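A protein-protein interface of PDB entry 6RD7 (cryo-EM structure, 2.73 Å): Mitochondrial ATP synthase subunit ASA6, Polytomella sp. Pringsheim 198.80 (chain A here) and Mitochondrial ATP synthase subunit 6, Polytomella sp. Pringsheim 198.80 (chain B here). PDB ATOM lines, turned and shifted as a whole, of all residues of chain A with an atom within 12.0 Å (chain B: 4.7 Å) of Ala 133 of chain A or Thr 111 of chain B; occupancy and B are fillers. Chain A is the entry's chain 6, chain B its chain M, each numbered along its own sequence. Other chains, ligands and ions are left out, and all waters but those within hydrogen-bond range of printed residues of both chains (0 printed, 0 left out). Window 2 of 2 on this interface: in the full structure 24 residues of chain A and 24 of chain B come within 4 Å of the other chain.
ND2 of Asn 108 of chain B lies within hydrogen-bond range of OG1 of Thr 136 of chain A, 3.4 Å away.
The backbone carbonyl oxygen (O) of Ala 133 of chain A lies within hydrogen-bond range of the side-chain hydroxyl (OG1) of Thr 136 of chain A (3.4 Å).
The side-chain hydroxyl (OG1) of Thr 136 of chain A lies within hydrogen-bond range of the backbone carbonyl oxygen (O) of Arg 130 of chain A.
NH2 of Arg 130 of chain A lies within hydrogen-bond range of OH of Tyr 126 of chain A (3.4 Å).
N of Ala 137 of chain A lies within hydrogen-bond range of O of Arg 130 of chain A (3.3 Å).
Phe 129 of chain A touches Asn 108 of chain B.
Phe 129 of chain A touches Phe 109 of chain B (CZ to CD1, 3.8 Å).
Arg 130 of chain A touches Asn 108 of chain B.
Met 132 of chain A touches Asn 108 of chain B (CB to O, 3.8 Å).
Phe 109 of chain B touches Met 132 of chain A (O to CE, 3.4 Å).
CE of Met 132 of chain A touches CA of Gly 112 of chain B, at 3.7 Å.
CB of Ala 133 of chain A touches ND2 of Asn 108 of chain B (3.6 Å).
CB of Ala 133 of chain A touches CB of Thr 111 of chain B (3.8 Å).
Arg 115 of chain B touches Pro 134 of chain A (NE to CG, 3.6 Å).
Thr 111 of chain B touches just one residue of chain A: Ala 133 (3.8 Å).
No residue of chain A comes within 4 Å of Thr 107 of chain B.
Asn 108 of chain B touches just these residues of chain A: Phe 129 (3.2 Å), Arg 130 (3.9 Å), Met 132 (3.8 Å), Ala 133 (3.6 Å) and Thr 136 (3.4 Å).
Phe 109 of chain B touches two residues of chain A.
No residue of chain A comes within 4 Å of Leu 110 of chain B.
Gly 112 of chain B touches one residue of chain A.
Of the printed residues of chain B, Pro 134 of chain A touches Arg 115 (3.6 Å).
Of the printed residues of chain B, Thr 136 of chain A touches Asn 108 (3.4 Å).
Leu 140 of chain A touches none of the printed residues of chain B.
The nearest residue of chain A that does not touch Thr 111 of chain B is Pro 134 of chain A (4.2 Å).
Of the 9 printed residues of chain B, 5 touch a printed residue of chain A.
Printed residues of chain B that touch a printed residue of chain A: Asn 108, Phe 109, Thr 111, Gly 112 and Arg 115.
Along chain B the printed residues that touch a printed residue of chain A span positions 108 to 115.
Among the printed residues, 10 pairs touch across the chains.
Among the printed residues, no Asp or Glu carboxylate lies within 4 Å of a Lys or Arg side-chain nitrogen of the other chain.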
ATOM      1  N   ALA A 124      36.815  13.124  35.790  1.00  0.00           N
ATOM      2  CA  ALA A 124      36.074  14.318  35.405  1.00  0.00           C
ATOM      3  C   ALA A 124      36.049  14.485  33.894  1.00  0.00           C
ATOM      4  O   ALA A 124      35.051  14.945  33.335  1.00  0.00           O
ATOM      5  CB  ALA A 124      36.681  15.548  36.072  1.00  0.00           C
ATOM      6  N   VAL A 125      37.120  14.073  33.214  1.00  0.00           N
ATOM      7  CA  VAL A 125      37.163  14.141  31.756  1.00  0.00           C
ATOM      8  C   VAL A 125      36.207  13.122  31.144  1.00  0.00           C
ATOM      9  O   VAL A 125      35.497  13.425  30.176  1.00  0.00           O
ATOM     10  CB  VAL A 125      38.613  13.950  31.272  1.00  0.00           C
ATOM     11  CG1 VAL A 125      38.682  13.690  29.779  1.00  0.00           C
ATOM     12  CG2 VAL A 125      39.428  15.173  31.617  1.00  0.00           C
ATOM     13  N   TYR A 126      36.141  11.918  31.726  1.00  0.00           N
ATOM     14  CA  TYR A 126      35.198  10.899  31.267  1.00  0.00           C
ATOM     15  C   TYR A 126      33.754  11.356  31.442  1.00  0.00           C
ATOM     16  O   TYR A 126      32.935  11.223  30.524  1.00  0.00           O
ATOM     17  CB  TYR A 126      35.436   9.590  32.025  1.00  0.00           C
ATOM     18  CG  TYR A 126      34.419   8.508  31.732  1.00  0.00           C
ATOM     19  CD1 TYR A 126      34.496   7.760  30.569  1.00  0.00           C
ATOM     20  CD2 TYR A 126      33.384   8.233  32.620  1.00  0.00           C
ATOM     21  CE1 TYR A 126      33.572   6.781  30.289  1.00  0.00           C
ATOM     22  CE2 TYR A 126      32.451   7.260  32.345  1.00  0.00           C
ATOM     23  CZ  TYR A 126      32.554   6.536  31.179  1.00  0.00           C
ATOM     24  OH  TYR A 126      31.637   5.554  30.898  1.00  0.00           O
ATOM     25  N   PHE A 127      33.431  11.923  32.601  1.00  0.00           N
ATOM     26  CA  PHE A 127      32.051  12.330  32.837  1.00  0.00           C
ATOM     27  C   PHE A 127      31.716  13.629  32.115  1.00  0.00           C
ATOM     28  O   PHE A 127      30.540  13.924  31.881  1.00  0.00           O
ATOM     29  CB  PHE A 127      31.793  12.446  34.334  1.00  0.00           C
ATOM     30  CG  PHE A 127      31.470  11.140  34.980  1.00  0.00           C
ATOM     31  CD1 PHE A 127      30.219  10.574  34.831  1.00  0.00           C
ATOM     32  CD2 PHE A 127      32.422  10.462  35.718  1.00  0.00           C
ATOM     33  CE1 PHE A 127      29.920   9.366  35.417  1.00  0.00           C
ATOM     34  CE2 PHE A 127      32.128   9.255  36.307  1.00  0.00           C
ATOM     35  CZ  PHE A 127      30.876   8.706  36.156  1.00  0.00           C
ATOM     36  N   ALA A 128      32.728  14.412  31.742  1.00  0.00           N
ATOM     37  CA  ALA A 128      32.479  15.586  30.916  1.00  0.00           C
ATOM     38  C   ALA A 128      32.252  15.189  29.471  1.00  0.00           C
ATOM     39  O   ALA A 128      31.489  15.841  28.751  1.00  0.00           O
ATOM     40  CB  ALA A 128      33.647  16.563  31.022  1.00  0.00           C
ATOM     41  N   PHE A 129      32.913  14.124  29.022  1.00  0.00           N
ATOM     42  CA  PHE A 129      32.659  13.627  27.677  1.00  0.00           C
ATOM     43  C   PHE A 129      31.306  12.936  27.609  1.00  0.00           C
ATOM     44  O   PHE A 129      30.653  12.951  26.562  1.00  0.00           O
ATOM     45  CB  PHE A 129      33.774  12.679  27.236  1.00  0.00           C
ATOM     46  CG  PHE A 129      35.018  13.374  26.737  1.00  0.00           C
ATOM     47  CD1 PHE A 129      35.172  14.745  26.844  1.00  0.00           C
ATOM     48  CD2 PHE A 129      36.036  12.644  26.160  1.00  0.00           C
ATOM     49  CE1 PHE A 129      36.311  15.368  26.389  1.00  0.00           C
ATOM     50  CE2 PHE A 129      37.180  13.261  25.704  1.00  0.00           C
ATOM     51  CZ  PHE A 129      37.316  14.624  25.818  1.00  0.00           C
ATOM     52  N   ARG A 130      30.858  12.354  28.725  1.00  0.00           N
ATOM     53  CA  ARG A 130      29.519  11.772  28.780  1.00  0.00           C
ATOM     54  C   ARG A 130      28.429  12.830  28.668  1.00  0.00           C
ATOM     55  O   ARG A 130      27.318  12.526  28.228  1.00  0.00           O
ATOM     56  CB  ARG A 130      29.342  10.982  30.074  1.00  0.00           C
ATOM     57  CG  ARG A 130      29.714   9.526  29.968  1.00  0.00           C
ATOM     58  CD  ARG A 130      29.360   8.775  31.234  1.00  0.00           C
ATOM     59  NE  ARG A 130      27.977   8.312  31.235  1.00  0.00           N
ATOM     60  CZ  ARG A 130      27.565   7.183  30.670  1.00  0.00           C
ATOM     61  NH1 ARG A 130      26.287   6.844  30.724  1.00  0.00           N
ATOM     62  NH2 ARG A 130      28.426   6.393  30.051  1.00  0.00           N
ATOM     63  N   GLY A 131      28.718  14.066  29.061  1.00  0.00           N
ATOM     64  CA  GLY A 131      27.768  15.146  28.909  1.00  0.00           C
ATOM     65  C   GLY A 131      27.734  15.795  27.548  1.00  0.00           C
ATOM     66  O   GLY A 131      26.845  16.604  27.282  1.00  0.00           O
ATOM     67  N   MET A 132      28.681  15.464  26.671  1.00  0.00           N
ATOM     68  CA  MET A 132      28.689  16.032  25.329  1.00  0.00           C
ATOM     69  C   MET A 132      27.645  15.366  24.446  1.00  0.00           C
ATOM     70  O   MET A 132      27.013  16.023  23.614  1.00  0.00           O
ATOM     71  CB  MET A 132      30.075  15.893  24.706  1.00  0.00           C
ATOM     72  CG  MET A 132      31.125  16.758  25.352  1.00  0.00           C
ATOM     73  SD  MET A 132      32.773  16.336  24.787  1.00  0.00           S
ATOM     74  CE  MET A 132      32.603  16.612  23.035  1.00  0.00           C
ATOM     75  N   ALA A 133      27.464  14.082  24.605  1.00  0.00           N
ATOM     76  CA  ALA A 133      26.442  13.360  23.866  1.00  0.00           C
ATOM     77  C   ALA A 133      25.135  13.396  24.638  1.00  0.00           C
ATOM     78  O   ALA A 133      25.132  13.123  25.841  1.00  0.00           O
ATOM     79  CB  ALA A 133      26.861  11.920  23.632  1.00  0.00           C
ATOM     80  N   PRO A 134      24.015  13.739  23.998  1.00  0.00           N
ATOM     81  CA  PRO A 134      22.733  13.729  24.718  1.00  0.00           C
ATOM     82  C   PRO A 134      22.248  12.341  25.091  1.00  0.00           C
ATOM     83  O   PRO A 134      21.398  12.219  25.977  1.00  0.00           O
ATOM     84  CB  PRO A 134      21.778  14.413  23.732  1.00  0.00           C
ATOM     85  CG  PRO A 134      22.651  15.200  22.844  1.00  0.00           C
ATOM     86  CD  PRO A 134      23.896  14.400  22.691  1.00  0.00           C
ATOM     87  N   ALA A 135      22.766  11.289  24.451  1.00  0.00           N
ATOM     88  CA  ALA A 135      22.351   9.932  24.789  1.00  0.00           C
ATOM     89  C   ALA A 135      22.886   9.492  26.143  1.00  0.00           C
ATOM     90  O   ALA A 135      22.285   8.635  26.795  1.00  0.00           O
ATOM     91  CB  ALA A 135      22.803   8.956  23.709  1.00  0.00           C
ATOM     92  N   THR A 136      24.008  10.053  26.579  1.00  0.00           N
ATOM     93  CA  THR A 136      24.580   9.712  27.868  1.00  0.00           C
ATOM     94  C   THR A 136      24.487  10.836  28.881  1.00  0.00           C
ATOM     95  O   THR A 136      24.821  10.622  30.049  1.00  0.00           O
ATOM     96  CB  THR A 136      26.047   9.299  27.708  1.00  0.00           C
ATOM     97  OG1 THR A 136      26.723  10.259  26.894  1.00  0.00           O
ATOM     98  CG2 THR A 136      26.131   7.957  27.045  1.00  0.00           C
ATOM     99  N   ALA A 137      24.045  12.022  28.468  1.00  0.00           N
ATOM    100  CA  ALA A 137      23.890  13.121  29.410  1.00  0.00           C
ATOM    101  C   ALA A 137      22.683  12.906  30.310  1.00  0.00           C
ATOM    102  O   ALA A 137      22.669  13.361  31.459  1.00  0.00           O
ATOM    103  CB  ALA A 137      23.771  14.442  28.656  1.00  0.00           C
ATOM    104  N   SER A 138      21.665  12.215  29.809  1.00  0.00           N
ATOM    105  CA  SER A 138      20.443  11.968  30.553  1.00  0.00           C
ATOM    106  C   SER A 138      20.200  10.474  30.666  1.00  0.00           C
ATOM    107  O   SER A 138      20.773   9.669  29.928  1.00  0.00           O
ATOM    108  CB  SER A 138      19.233  12.631  29.884  1.00  0.00           C
ATOM    109  OG  SER A 138      19.374  14.037  29.845  1.00  0.00           O
ATOM    110  N   THR A 139      19.341  10.112  31.611  1.00  0.00           N
ATOM    111  CA  THR A 139      18.789   8.769  31.651  1.00  0.00           C
ATOM    112  C   THR A 139      17.786   8.615  30.514  1.00  0.00           C
ATOM    113  O   THR A 139      17.052   9.548  30.181  1.00  0.00           O
ATOM    114  CB  THR A 139      18.126   8.517  33.011  1.00  0.00           C
ATOM    115  OG1 THR A 139      19.082   8.747  34.052  1.00  0.00           O
ATOM    116  CG2 THR A 139      17.608   7.087  33.143  1.00  0.00           C
ATOM    117  N   LEU A 140      17.794   7.439  29.881  1.00  0.00           N
ATOM    118  CA  LEU A 140      16.840   7.123  28.828  1.00  0.00           C
ATOM    119  C   LEU A 140      15.420   7.112  29.370  1.00  0.00           C
ATOM    120  O   LEU A 140      15.038   6.208  30.118  1.00  0.00           O
ATOM    121  CB  LEU A 140      17.168   5.772  28.198  1.00  0.00           C
ATOM    122  CG  LEU A 140      16.196   5.299  27.125  1.00  0.00           C
ATOM    123  CD1 LEU A 140      16.324   6.134  25.880  1.00  0.00           C
ATOM    124  CD2 LEU A 140      16.455   3.865  26.817  1.00  0.00           C
ATOM    125  N   THR B 107      32.644   7.696  21.038  1.00  0.00           N
ATOM    126  CA  THR B 107      31.323   7.978  20.490  1.00  0.00           C
ATOM    127  C   THR B 107      30.725   9.237  21.102  1.00  0.00           C
ATOM    128  O   THR B 107      30.146  10.063  20.393  1.00  0.00           O
ATOM    129  CB  THR B 107      30.400   6.787  20.726  1.00  0.00           C
ATOM    130  OG1 THR B 107      31.067   5.584  20.332  1.00  0.00           O
ATOM    131  CG2 THR B 107      29.121   6.928  19.939  1.00  0.00           C
ATOM    132  N   ASN B 108      30.894   9.416  22.412  1.00  0.00           N
ATOM    133  CA  ASN B 108      30.363  10.593  23.089  1.00  0.00           C
ATOM    134  C   ASN B 108      31.101  11.857  22.673  1.00  0.00           C
ATOM    135  O   ASN B 108      30.473  12.893  22.407  1.00  0.00           O
ATOM    136  CB  ASN B 108      30.458  10.404  24.599  1.00  0.00           C
ATOM    137  CG  ASN B 108      29.613   9.266  25.102  1.00  0.00           C
ATOM    138  OD1 ASN B 108      29.871   8.721  26.170  1.00  0.00           O
ATOM    139  ND2 ASN B 108      28.593   8.901  24.341  1.00  0.00           N
ATOM    140  N   PHE B 109      32.434  11.783  22.607  1.00  0.00           N
ATOM    141  CA  PHE B 109      33.236  12.926  22.188  1.00  0.00           C
ATOM    142  C   PHE B 109      32.936  13.310  20.746  1.00  0.00           C
ATOM    143  O   PHE B 109      32.815  14.494  20.417  1.00  0.00           O
ATOM    144  CB  PHE B 109      34.720  12.603  22.365  1.00  0.00           C
ATOM    145  CG  PHE B 109      35.640  13.614  21.753  1.00  0.00           C
ATOM    146  CD1 PHE B 109      35.821  14.850  22.345  1.00  0.00           C
ATOM    147  CD2 PHE B 109      36.333  13.324  20.590  1.00  0.00           C
ATOM    148  CE1 PHE B 109      36.665  15.779  21.787  1.00  0.00           C
ATOM    149  CE2 PHE B 109      37.177  14.251  20.027  1.00  0.00           C
ATOM    150  CZ  PHE B 109      37.344  15.480  20.628  1.00  0.00           C
ATOM    151  N   LEU B 110      32.756  12.315  19.881  1.00  0.00           N
ATOM    152  CA  LEU B 110      32.511  12.600  18.477  1.00  0.00           C
ATOM    153  C   LEU B 110      31.087  13.078  18.249  1.00  0.00           C
ATOM    154  O   LEU B 110      30.838  13.871  17.335  1.00  0.00           O
ATOM    155  CB  LEU B 110      32.808  11.355  17.661  1.00  0.00           C
ATOM    156  CG  LEU B 110      33.267  11.530  16.227  1.00  0.00           C
ATOM    157  CD1 LEU B 110      34.431  12.491  16.149  1.00  0.00           C
ATOM    158  CD2 LEU B 110      33.679  10.174  15.755  1.00  0.00           C
ATOM    159  N   THR B 111      30.147  12.629  19.085  1.00  0.00           N
ATOM    160  CA  THR B 111      28.791  13.160  19.053  1.00  0.00           C
ATOM    161  C   THR B 111      28.776  14.631  19.424  1.00  0.00           C
ATOM    162  O   THR B 111      28.146  15.443  18.737  1.00  0.00           O
ATOM    163  CB  THR B 111      27.900  12.376  20.011  1.00  0.00           C
ATOM    164  OG1 THR B 111      28.077  10.975  19.791  1.00  0.00           O
ATOM    165  CG2 THR B 111      26.449  12.735  19.796  1.00  0.00           C
ATOM    166  N   GLY B 112      29.486  14.993  20.496  1.00  0.00           N
ATOM    167  CA  GLY B 112      29.561  16.393  20.887  1.00  0.00           C
ATOM    168  C   GLY B 112      30.267  17.261  19.864  1.00  0.00           C
ATOM    169  O   GLY B 112      29.844  18.389  19.602  1.00  0.00           O
ATOM    170  N   VAL B 113      31.316  16.727  19.230  1.00  0.00           N
ATOM    171  CA  VAL B 113      32.057  17.478  18.218  1.00  0.00           C
ATOM    172  C   VAL B 113      31.199  17.700  16.974  1.00  0.00           C
ATOM    173  O   VAL B 113      31.126  18.819  16.445  1.00  0.00           O
ATOM    174  CB  VAL B 113      33.378  16.758  17.890  1.00  0.00           C
ATOM    175  CG1 VAL B 113      33.933  17.183  16.549  1.00  0.00           C
ATOM    176  CG2 VAL B 113      34.398  17.029  18.966  1.00  0.00           C
ATOM    177  N   TYR B 114      30.512  16.648  16.510  1.00  0.00           N
ATOM    178  CA  TYR B 114      29.654  16.779  15.336  1.00  0.00           C
ATOM    179  C   TYR B 114      28.478  17.705  15.604  1.00  0.00           C
ATOM    180  O   TYR B 114      28.081  18.476  14.727  1.00  0.00           O
ATOM    181  CB  TYR B 114      29.142  15.412  14.884  1.00  0.00           C
ATOM    182  CG  TYR B 114      28.140  15.520  13.756  1.00  0.00           C
ATOM    183  CD1 TYR B 114      28.558  15.836  12.474  1.00  0.00           C
ATOM    184  CD2 TYR B 114      26.780  15.332  13.975  1.00  0.00           C
ATOM    185  CE1 TYR B 114      27.661  15.955  11.444  1.00  0.00           C
ATOM    186  CE2 TYR B 114      25.873  15.457  12.947  1.00  0.00           C
ATOM    187  CZ  TYR B 114      26.323  15.767  11.684  1.00  0.00           C
ATOM    188  OH  TYR B 114      25.434  15.886  10.645  1.00  0.00           O
ATOM    189  N   ARG B 115      27.908  17.647  16.807  1.00  0.00           N
ATOM    190  CA  ARG B 115      26.783  18.519  17.113  1.00  0.00           C
ATOM    191  C   ARG B 115      27.241  19.952  17.325  1.00  0.00           C
ATOM    192  O   ARG B 115      26.451  20.888  17.177  1.00  0.00           O
ATOM    193  CB  ARG B 115      26.039  17.998  18.334  1.00  0.00           C
ATOM    194  CG  ARG B 115      25.211  16.781  18.046  1.00  0.00           C
ATOM    195  CD  ARG B 115      24.664  16.203  19.320  1.00  0.00           C
ATOM    196  NE  ARG B 115      23.825  17.164  20.019  1.00  0.00           N
ATOM    197  CZ  ARG B 115      22.532  17.339  19.779  1.00  0.00           C
ATOM    198  NH1 ARG B 115      21.851  18.240  20.466  1.00  0.00           N
ATOM    199  NH2 ARG B 115      21.921  16.615  18.855  1.00  0.00           N
